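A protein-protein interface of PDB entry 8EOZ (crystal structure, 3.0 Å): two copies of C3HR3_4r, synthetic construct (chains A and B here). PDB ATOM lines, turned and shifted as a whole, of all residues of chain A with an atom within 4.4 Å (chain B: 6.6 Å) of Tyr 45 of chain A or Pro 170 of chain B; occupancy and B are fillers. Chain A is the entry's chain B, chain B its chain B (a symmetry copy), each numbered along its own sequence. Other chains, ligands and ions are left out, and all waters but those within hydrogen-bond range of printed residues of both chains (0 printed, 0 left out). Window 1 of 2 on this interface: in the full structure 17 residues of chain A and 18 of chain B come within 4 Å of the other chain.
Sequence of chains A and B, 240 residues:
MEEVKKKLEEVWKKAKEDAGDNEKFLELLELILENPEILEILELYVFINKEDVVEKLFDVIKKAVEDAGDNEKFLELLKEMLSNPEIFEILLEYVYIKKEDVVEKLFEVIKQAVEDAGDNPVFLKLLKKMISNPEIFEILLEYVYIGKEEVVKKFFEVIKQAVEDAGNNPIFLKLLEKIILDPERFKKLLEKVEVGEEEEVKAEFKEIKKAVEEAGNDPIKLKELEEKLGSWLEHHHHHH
The backbone carbonyl oxygen of Ile 48 of chain A lies close to the side-chain amide nitrogen of Asn 168 of chain B, 3.4 Å away.
ND2 of Asn 168 of chain B lies close to ND2 of Asn 49 of chain A (3.2 Å).
The backbone carbonyl oxygen (O) of Asn 168 of chain B sits at hydrogen-bond distance from the side-chain amino group (NZ) of Lys 50 of chain A (2.5 Å).
O of Tyr 45 of chain A lies within hydrogen-bond range of N of Lys 50 of chain A, at 3.0 Å.
O of Tyr 45 of chain A is in hydrogen-bond range of N of Glu 51 of chain A (3.5 Å).
The side-chain amino group (NZ) of Lys 50 of chain A sits at hydrogen-bond distance from the backbone carbonyl oxygen (O) of Ile 48 of chain A (2.9 Å).
The side-chain amide oxygen (OD1) of Asn 169 of chain B is in hydrogen-bond range of the backbone NH (N) of Ile 171 of chain B (3.0 Å).
Among the printed residues, merely in contact across the chains: Tyr 45 of chain A with Pro 170 of chain B (3.2 Å), Ile 48 of chain A with Pro 170 of chain B (3.9 Å), Ile 48 of chain A with Leu 173 of chain B (3.6 Å), Lys 50 of chain A with Pro 170 of chain B (3.7 Å), Glu 93 of chain A with Ile 171 of chain B (3.8 Å), Glu 93 of chain A with Lys 174 of chain B (3.4 Å), Tyr 96 of chain A with Asn 169 of chain B (3.2 Å), Tyr 96 of chain A with Pro 170 of chain B (3.6 Å) and Tyr 96 of chain A with Ile 171 of chain B (3.9 Å).
Of chain B, only Pro 170 (3.2 Å) comes within 4 Å of Tyr 45 of chain A.
Printed residues of chain A within 4 Å of Pro 170 of chain B: Tyr 45 (3.2 Å), Ile 48 (3.9 Å), Lys 50 (3.7 Å) and Tyr 96 (3.6 Å).
Printed residues of chain A within 4 Å of Asn 168 of chain B: Ile 48, Asn 49 and Lys 50.
Of the printed residues of chain A, Ile 171 of chain B touches Glu 93 (3.8 Å) and Tyr 96 (3.9 Å).
Of the printed residues of chain B, Tyr 96 of chain A touches Asn 169 (3.2 Å), Pro 170 (3.6 Å) and Ile 171 (3.9 Å).
Val 54 of chain A touches none of the printed residues of chain B.
Phe 172 of chain B touches none of the printed residues of chain A.
Hydrophobic or aromatic side chains of chain B that line the printed part of chain A: Pro 170, Ile 171 and Leu 173.
Among the printed residues, 12 pairs touch across the chains.
Among the printed residues, no Asp or Glu carboxylate lies within 4 Å of a Lys or Arg side-chain nitrogen of the other chain.
No position is printed for both chains.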
ATOM      1  N   ILE A  41      29.055   7.450 -32.750  1.00  0.00           N
ATOM      2  CA  ILE A  41      29.440   7.560 -31.346  1.00  0.00           C
ATOM      3  C   ILE A  41      30.294   8.801 -31.126  1.00  0.00           C
ATOM      4  O   ILE A  41      30.125   9.520 -30.135  1.00  0.00           O
ATOM      5  CB  ILE A  41      30.172   6.287 -30.891  1.00  0.00           C
ATOM      6  CG1 ILE A  41      29.421   5.041 -31.355  1.00  0.00           C
ATOM      7  CG2 ILE A  41      30.319   6.274 -29.377  1.00  0.00           C
ATOM      8  CD1 ILE A  41      30.126   3.749 -31.005  1.00  0.00           C
ATOM      9  N   LEU A  42      31.223   9.073 -32.047  1.00  0.00           N
ATOM     10  CA  LEU A  42      32.076  10.251 -31.919  1.00  0.00           C
ATOM     11  C   LEU A  42      31.261  11.536 -31.998  1.00  0.00           C
ATOM     12  O   LEU A  42      31.540  12.501 -31.276  1.00  0.00           O
ATOM     13  CB  LEU A  42      33.155  10.231 -33.001  1.00  0.00           C
ATOM     14  CG  LEU A  42      34.046   8.987 -33.043  1.00  0.00           C
ATOM     15  CD1 LEU A  42      35.023   9.061 -34.208  1.00  0.00           C
ATOM     16  CD2 LEU A  42      34.790   8.818 -31.728  1.00  0.00           C
ATOM     17  N   GLU A  43      30.248  11.568 -32.869  1.00  0.00           N
ATOM     18  CA  GLU A  43      29.414  12.758 -33.001  1.00  0.00           C
ATOM     19  C   GLU A  43      28.554  12.984 -31.763  1.00  0.00           C
ATOM     20  O   GLU A  43      28.284  14.133 -31.399  1.00  0.00           O
ATOM     21  CB  GLU A  43      28.533  12.647 -34.246  1.00  0.00           C
ATOM     22  CG  GLU A  43      29.314  12.538 -35.545  1.00  0.00           C
ATOM     23  CD  GLU A  43      28.428  12.306 -36.752  1.00  0.00           C
ATOM     24  OE1 GLU A  43      27.246  11.948 -36.567  1.00  0.00           O
ATOM     25  OE2 GLU A  43      28.915  12.483 -37.889  1.00  0.00           O
ATOM     26  N   LEU A  44      28.107  11.909 -31.110  1.00  0.00           N
ATOM     27  CA  LEU A  44      27.392  12.064 -29.851  1.00  0.00           C
ATOM     28  C   LEU A  44      28.321  12.460 -28.714  1.00  0.00           C
ATOM     29  O   LEU A  44      27.857  13.029 -27.722  1.00  0.00           O
ATOM     30  CB  LEU A  44      26.656  10.772 -29.495  1.00  0.00           C
ATOM     31  CG  LEU A  44      25.496  10.382 -30.409  1.00  0.00           C
ATOM     32  CD1 LEU A  44      24.860   9.089 -29.935  1.00  0.00           C
ATOM     33  CD2 LEU A  44      24.471  11.497 -30.469  1.00  0.00           C
ATOM     34  N   TYR A  45      29.616  12.180 -28.840  1.00  0.00           N
ATOM     35  CA  TYR A  45      30.576  12.506 -27.795  1.00  0.00           C
ATOM     36  C   TYR A  45      31.138  13.916 -27.912  1.00  0.00           C
ATOM     37  O   TYR A  45      31.771  14.389 -26.964  1.00  0.00           O
ATOM     38  CB  TYR A  45      31.722  11.487 -27.789  1.00  0.00           C
ATOM     39  CG  TYR A  45      31.514  10.363 -26.797  1.00  0.00           C
ATOM     40  CD1 TYR A  45      30.545   9.392 -27.009  1.00  0.00           C
ATOM     41  CD2 TYR A  45      32.281  10.279 -25.641  1.00  0.00           C
ATOM     42  CE1 TYR A  45      30.345   8.367 -26.102  1.00  0.00           C
ATOM     43  CE2 TYR A  45      32.090   9.256 -24.727  1.00  0.00           C
ATOM     44  CZ  TYR A  45      31.121   8.302 -24.964  1.00  0.00           C
ATOM     45  OH  TYR A  45      30.925   7.280 -24.062  1.00  0.00           O
ATOM     46  N   VAL A  46      30.932  14.600 -29.034  1.00  0.00           N
ATOM     47  CA  VAL A  46      31.324  16.002 -29.108  1.00  0.00           C
ATOM     48  C   VAL A  46      30.167  16.920 -28.716  1.00  0.00           C
ATOM     49  O   VAL A  46      30.396  17.992 -28.144  1.00  0.00           O
ATOM     50  CB  VAL A  46      31.867  16.348 -30.507  1.00  0.00           C
ATOM     51  CG1 VAL A  46      33.166  15.597 -30.766  1.00  0.00           C
ATOM     52  CG2 VAL A  46      30.846  16.026 -31.584  1.00  0.00           C
ATOM     53  N   PHE A  47      28.927  16.517 -29.004  1.00  0.00           N
ATOM     54  CA  PHE A  47      27.768  17.239 -28.494  1.00  0.00           C
ATOM     55  C   PHE A  47      27.641  17.105 -26.982  1.00  0.00           C
ATOM     56  O   PHE A  47      27.026  17.965 -26.342  1.00  0.00           O
ATOM     57  CB  PHE A  47      26.496  16.735 -29.181  1.00  0.00           C
ATOM     58  CG  PHE A  47      25.225  17.287 -28.599  1.00  0.00           C
ATOM     59  CD1 PHE A  47      24.761  18.536 -28.974  1.00  0.00           C
ATOM     60  CD2 PHE A  47      24.489  16.549 -27.686  1.00  0.00           C
ATOM     61  CE1 PHE A  47      23.590  19.044 -28.442  1.00  0.00           C
ATOM     62  CE2 PHE A  47      23.319  17.051 -27.149  1.00  0.00           C
ATOM     63  CZ  PHE A  47      22.868  18.302 -27.529  1.00  0.00           C
ATOM     64  N   ILE A  48      28.227  16.059 -26.399  1.00  0.00           N
ATOM     65  CA  ILE A  48      28.163  15.818 -24.963  1.00  0.00           C
ATOM     66  C   ILE A  48      29.351  16.499 -24.288  1.00  0.00           C
ATOM     67  O   ILE A  48      29.578  16.334 -23.085  1.00  0.00           O
ATOM     68  CB  ILE A  48      28.116  14.302 -24.676  1.00  0.00           C
ATOM     69  CG1 ILE A  48      27.441  14.013 -23.337  1.00  0.00           C
ATOM     70  CG2 ILE A  48      29.504  13.701 -24.683  1.00  0.00           C
ATOM     71  CD1 ILE A  48      27.437  12.540 -22.967  1.00  0.00           C
ATOM     72  N   ASN A  49      30.112  17.271 -25.069  1.00  0.00           N
ATOM     73  CA  ASN A  49      31.213  18.104 -24.577  1.00  0.00           C
ATOM     74  C   ASN A  49      32.392  17.284 -24.058  1.00  0.00           C
ATOM     75  O   ASN A  49      33.111  17.723 -23.155  1.00  0.00           O
ATOM     76  CB  ASN A  49      30.740  19.087 -23.497  1.00  0.00           C
ATOM     77  CG  ASN A  49      29.963  20.257 -24.071  1.00  0.00           C
ATOM     78  OD1 ASN A  49      30.413  20.919 -25.007  1.00  0.00           O
ATOM     79  ND2 ASN A  49      28.786  20.515 -23.513  1.00  0.00           N
ATOM     80  N   LYS A  50      32.615  16.094 -24.614  1.00  0.00           N
ATOM     81  CA  LYS A  50      33.822  15.350 -24.284  1.00  0.00           C
ATOM     82  C   LYS A  50      34.977  15.826 -25.154  1.00  0.00           C
ATOM     83  O   LYS A  50      35.786  16.650 -24.714  1.00  0.00           O
ATOM     84  CB  LYS A  50      33.607  13.844 -24.445  1.00  0.00           C
ATOM     85  CG  LYS A  50      32.691  13.250 -23.391  1.00  0.00           C
ATOM     86  CD  LYS A  50      33.120  13.676 -21.997  1.00  0.00           C
ATOM     87  CE  LYS A  50      31.999  13.500 -20.992  1.00  0.00           C
ATOM     88  NZ  LYS A  50      30.817  14.335 -21.332  1.00  0.00           N
ATOM     89  N   GLU A  51      35.062  15.310 -26.383  1.00  0.00           N
ATOM     90  CA  GLU A  51      36.102  15.689 -27.339  1.00  0.00           C
ATOM     91  C   GLU A  51      37.488  15.286 -26.846  1.00  0.00           C
ATOM     92  O   GLU A  51      38.233  14.616 -27.567  1.00  0.00           O
ATOM     93  CB  GLU A  51      36.048  17.192 -27.631  1.00  0.00           C
ATOM     94  CG  GLU A  51      34.679  17.677 -28.077  1.00  0.00           C
ATOM     95  CD  GLU A  51      34.288  19.002 -27.448  1.00  0.00           C
ATOM     96  OE1 GLU A  51      35.194  19.771 -27.061  1.00  0.00           O
ATOM     97  OE2 GLU A  51      33.073  19.272 -27.336  1.00  0.00           O
ATOM     98  N   VAL A  53      37.906  13.168 -24.491  1.00  0.00           N
ATOM     99  CA  VAL A  53      37.780  11.717 -24.373  1.00  0.00           C
ATOM    100  C   VAL A  53      38.055  11.056 -25.715  1.00  0.00           C
ATOM    101  O   VAL A  53      38.718  10.012 -25.790  1.00  0.00           O
ATOM    102  CB  VAL A  53      36.389  11.343 -23.828  1.00  0.00           C
ATOM    103  CG1 VAL A  53      36.167   9.841 -23.914  1.00  0.00           C
ATOM    104  CG2 VAL A  53      36.239  11.824 -22.396  1.00  0.00           C
ATOM    105  N   VAL A  54      37.558  11.654 -26.799  1.00  0.00           N
ATOM    106  CA  VAL A  54      37.878  11.160 -28.132  1.00  0.00           C
ATOM    107  C   VAL A  54      39.337  11.444 -28.466  1.00  0.00           C
ATOM    108  O   VAL A  54      40.012  10.631 -29.109  1.00  0.00           O
ATOM    109  CB  VAL A  54      36.922  11.779 -29.169  1.00  0.00           C
ATOM    110  CG1 VAL A  54      37.281  11.316 -30.573  1.00  0.00           C
ATOM    111  CG2 VAL A  54      35.480  11.425 -28.836  1.00  0.00           C
ATOM    112  N   LEU A  92      35.675   4.318 -25.044  1.00  0.00           N
ATOM    113  CA  LEU A  92      35.390   5.715 -24.743  1.00  0.00           C
ATOM    114  C   LEU A  92      34.896   5.890 -23.315  1.00  0.00           C
ATOM    115  O   LEU A  92      35.090   6.953 -22.714  1.00  0.00           O
ATOM    116  CB  LEU A  92      34.363   6.267 -25.733  1.00  0.00           C
ATOM    117  CG  LEU A  92      34.877   6.577 -27.138  1.00  0.00           C
ATOM    118  CD1 LEU A  92      33.722   6.807 -28.099  1.00  0.00           C
ATOM    119  CD2 LEU A  92      35.795   7.793 -27.111  1.00  0.00           C
ATOM    120  N   GLU A  93      34.255   4.864 -22.753  1.00  0.00           N
ATOM    121  CA  GLU A  93      33.818   4.928 -21.366  1.00  0.00           C
ATOM    122  C   GLU A  93      34.921   4.547 -20.393  1.00  0.00           C
ATOM    123  O   GLU A  93      34.824   4.875 -19.207  1.00  0.00           O
ATOM    124  CB  GLU A  93      32.598   4.033 -21.159  1.00  0.00           C
ATOM    125  CG  GLU A  93      31.364   4.549 -21.877  1.00  0.00           C
ATOM    126  CD  GLU A  93      30.255   3.525 -21.942  1.00  0.00           C
ATOM    127  OE1 GLU A  93      30.463   2.387 -21.468  1.00  0.00           O
ATOM    128  OE2 GLU A  93      29.175   3.857 -22.473  1.00  0.00           O
ATOM    129  N   TYR A  96      36.640   8.358 -20.164  1.00  0.00           N
ATOM    130  CA  TYR A  96      35.953   9.321 -19.315  1.00  0.00           C
ATOM    131  C   TYR A  96      36.138   8.971 -17.844  1.00  0.00           C
ATOM    132  O   TYR A  96      36.244   9.861 -16.992  1.00  0.00           O
ATOM    133  CB  TYR A  96      34.474   9.376 -19.688  1.00  0.00           C
ATOM    134  CG  TYR A  96      33.620  10.180 -18.735  1.00  0.00           C
ATOM    135  CD1 TYR A  96      33.724  11.566 -18.670  1.00  0.00           C
ATOM    136  CD2 TYR A  96      32.695   9.556 -17.908  1.00  0.00           C
ATOM    137  CE1 TYR A  96      32.930  12.309 -17.802  1.00  0.00           C
ATOM    138  CE2 TYR A  96      31.896  10.288 -17.038  1.00  0.00           C
ATOM    139  CZ  TYR A  96      32.017  11.664 -16.991  1.00  0.00           C
ATOM    140  OH  TYR A  96      31.231  12.400 -16.132  1.00  0.00           O
ATOM    141  N   ALA B 166      21.478  14.578 -17.352  1.00  0.00           N
ATOM    142  CA  ALA B 166      22.561  13.613 -17.264  1.00  0.00           C
ATOM    143  C   ALA B 166      23.908  14.237 -16.934  1.00  0.00           C
ATOM    144  O   ALA B 166      24.848  13.496 -16.626  1.00  0.00           O
ATOM    145  CB  ALA B 166      22.685  12.824 -18.576  1.00  0.00           C
ATOM    146  N   GLY B 167      24.025  15.563 -16.971  1.00  0.00           N
ATOM    147  CA  GLY B 167      25.304  16.208 -16.733  1.00  0.00           C
ATOM    148  C   GLY B 167      26.357  15.858 -17.759  1.00  0.00           C
ATOM    149  O   GLY B 167      27.552  15.878 -17.440  1.00  0.00           O
ATOM    150  N   ASN B 168      25.944  15.523 -18.986  1.00  0.00           N
ATOM    151  CA  ASN B 168      26.856  15.102 -20.053  1.00  0.00           C
ATOM    152  C   ASN B 168      27.651  13.856 -19.671  1.00  0.00           C
ATOM    153  O   ASN B 168      28.740  13.620 -20.197  1.00  0.00           O
ATOM    154  CB  ASN B 168      27.810  16.230 -20.458  1.00  0.00           C
ATOM    155  CG  ASN B 168      27.106  17.360 -21.178  1.00  0.00           C
ATOM    156  OD1 ASN B 168      26.015  17.180 -21.720  1.00  0.00           O
ATOM    157  ND2 ASN B 168      27.730  18.532 -21.194  1.00  0.00           N
ATOM    158  N   ASN B 169      27.114  13.056 -18.757  1.00  0.00           N
ATOM    159  CA  ASN B 169      27.773  11.844 -18.293  1.00  0.00           C
ATOM    160  C   ASN B 169      27.465  10.701 -19.252  1.00  0.00           C
ATOM    161  O   ASN B 169      26.321  10.229 -19.311  1.00  0.00           O
ATOM    162  CB  ASN B 169      27.318  11.500 -16.871  1.00  0.00           C
ATOM    163  CG  ASN B 169      28.204  10.467 -16.201  1.00  0.00           C
ATOM    164  OD1 ASN B 169      28.819   9.631 -16.862  1.00  0.00           O
ATOM    165  ND2 ASN B 169      28.271  10.519 -14.875  1.00  0.00           N
ATOM    166  N   PRO B 170      28.451  10.231 -20.021  1.00  0.00           N
ATOM    167  CA  PRO B 170      28.177   9.139 -20.965  1.00  0.00           C
ATOM    168  C   PRO B 170      27.849   7.823 -20.289  1.00  0.00           C
ATOM    169  O   PRO B 170      27.207   6.972 -20.915  1.00  0.00           O
ATOM    170  CB  PRO B 170      29.477   9.041 -21.772  1.00  0.00           C
ATOM    171  CG  PRO B 170      30.524   9.538 -20.833  1.00  0.00           C
ATOM    172  CD  PRO B 170      29.867  10.637 -20.043  1.00  0.00           C
ATOM    173  N   ILE B 171      28.267   7.628 -19.037  1.00  0.00           N
ATOM    174  CA  ILE B 171      27.986   6.375 -18.344  1.00  0.00           C
ATOM    175  C   ILE B 171      26.490   6.234 -18.087  1.00  0.00           C
ATOM    176  O   ILE B 171      25.895   5.183 -18.350  1.00  0.00           O
ATOM    177  CB  ILE B 171      28.791   6.294 -17.035  1.00  0.00           C
ATOM    178  CG1 ILE B 171      30.275   6.571 -17.296  1.00  0.00           C
ATOM    179  CG2 ILE B 171      28.605   4.932 -16.380  1.00  0.00           C
ATOM    180  CD1 ILE B 171      30.970   5.503 -18.113  1.00  0.00           C
ATOM    181  N   PHE B 172      25.860   7.295 -17.577  1.00  0.00           N
ATOM    182  CA  PHE B 172      24.438   7.221 -17.258  1.00  0.00           C
ATOM    183  C   PHE B 172      23.575   7.186 -18.511  1.00  0.00           C
ATOM    184  O   PHE B 172      22.493   6.589 -18.498  1.00  0.00           O
ATOM    185  CB  PHE B 172      24.033   8.398 -16.369  1.00  0.00           C
ATOM    186  CG  PHE B 172      22.574   8.416 -16.027  1.00  0.00           C
ATOM    187  CD1 PHE B 172      22.058   7.532 -15.095  1.00  0.00           C
ATOM    188  CD2 PHE B 172      21.714   9.313 -16.641  1.00  0.00           C
ATOM    189  CE1 PHE B 172      20.712   7.541 -14.781  1.00  0.00           C
ATOM    190  CE2 PHE B 172      20.367   9.330 -16.332  1.00  0.00           C
ATOM    191  CZ  PHE B 172      19.865   8.442 -15.400  1.00  0.00           C
ATOM    192  N   LEU B 173      24.023   7.819 -19.598  1.00  0.00           N
ATOM    193  CA  LEU B 173      23.264   7.764 -20.844  1.00  0.00           C
ATOM    194  C   LEU B 173      23.269   6.358 -21.431  1.00  0.00           C
ATOM    195  O   LEU B 173      22.259   5.908 -21.986  1.00  0.00           O
ATOM    196  CB  LEU B 173      23.824   8.772 -21.847  1.00  0.00           C
ATOM    197  CG  LEU B 173      23.537  10.244 -21.542  1.00  0.00           C
ATOM    198  CD1 LEU B 173      24.111  11.141 -22.624  1.00  0.00           C
ATOM    199  CD2 LEU B 173      22.041  10.470 -21.395  1.00  0.00           C
ATOM    200  N   LYS B 174      24.393   5.648 -21.319  1.00  0.00           N
ATOM    201  CA  LYS B 174      24.431   4.260 -21.767  1.00  0.00           C
ATOM    202  C   LYS B 174      23.566   3.377 -20.877  1.00  0.00           C
ATOM    203  O   LYS B 174      22.914   2.445 -21.363  1.00  0.00           O
ATOM    204  CB  LYS B 174      25.871   3.751 -21.790  1.00  0.00           C
ATOM    205  CG  LYS B 174      26.028   2.399 -22.463  1.00  0.00           C
ATOM    206  CD  LYS B 174      25.846   2.516 -23.966  1.00  0.00           C
ATOM    207  CE  LYS B 174      25.765   1.150 -24.621  1.00  0.00           C
ATOM    208  NZ  LYS B 174      24.466   0.488 -24.333  1.00  0.00           N
ATOM    209  N   LEU B 175      23.551   3.654 -19.572  1.00  0.00           N
ATOM    210  CA  LEU B 175      22.680   2.910 -18.667  1.00  0.00           C
ATOM    211  C   LEU B 175      21.213   3.223 -18.934  1.00  0.00           C
ATOM    212  O   LEU B 175      20.364   2.326 -18.883  1.00  0.00           O
ATOM    213  CB  LEU B 175      23.042   3.222 -17.217  1.00  0.00           C
ATOM    214  CG  LEU B 175      24.416   2.724 -16.771  1.00  0.00           C
ATOM    215  CD1 LEU B 175      24.701   3.145 -15.343  1.00  0.00           C
ATOM    216  CD2 LEU B 175      24.500   1.214 -16.915  1.00  0.00           C
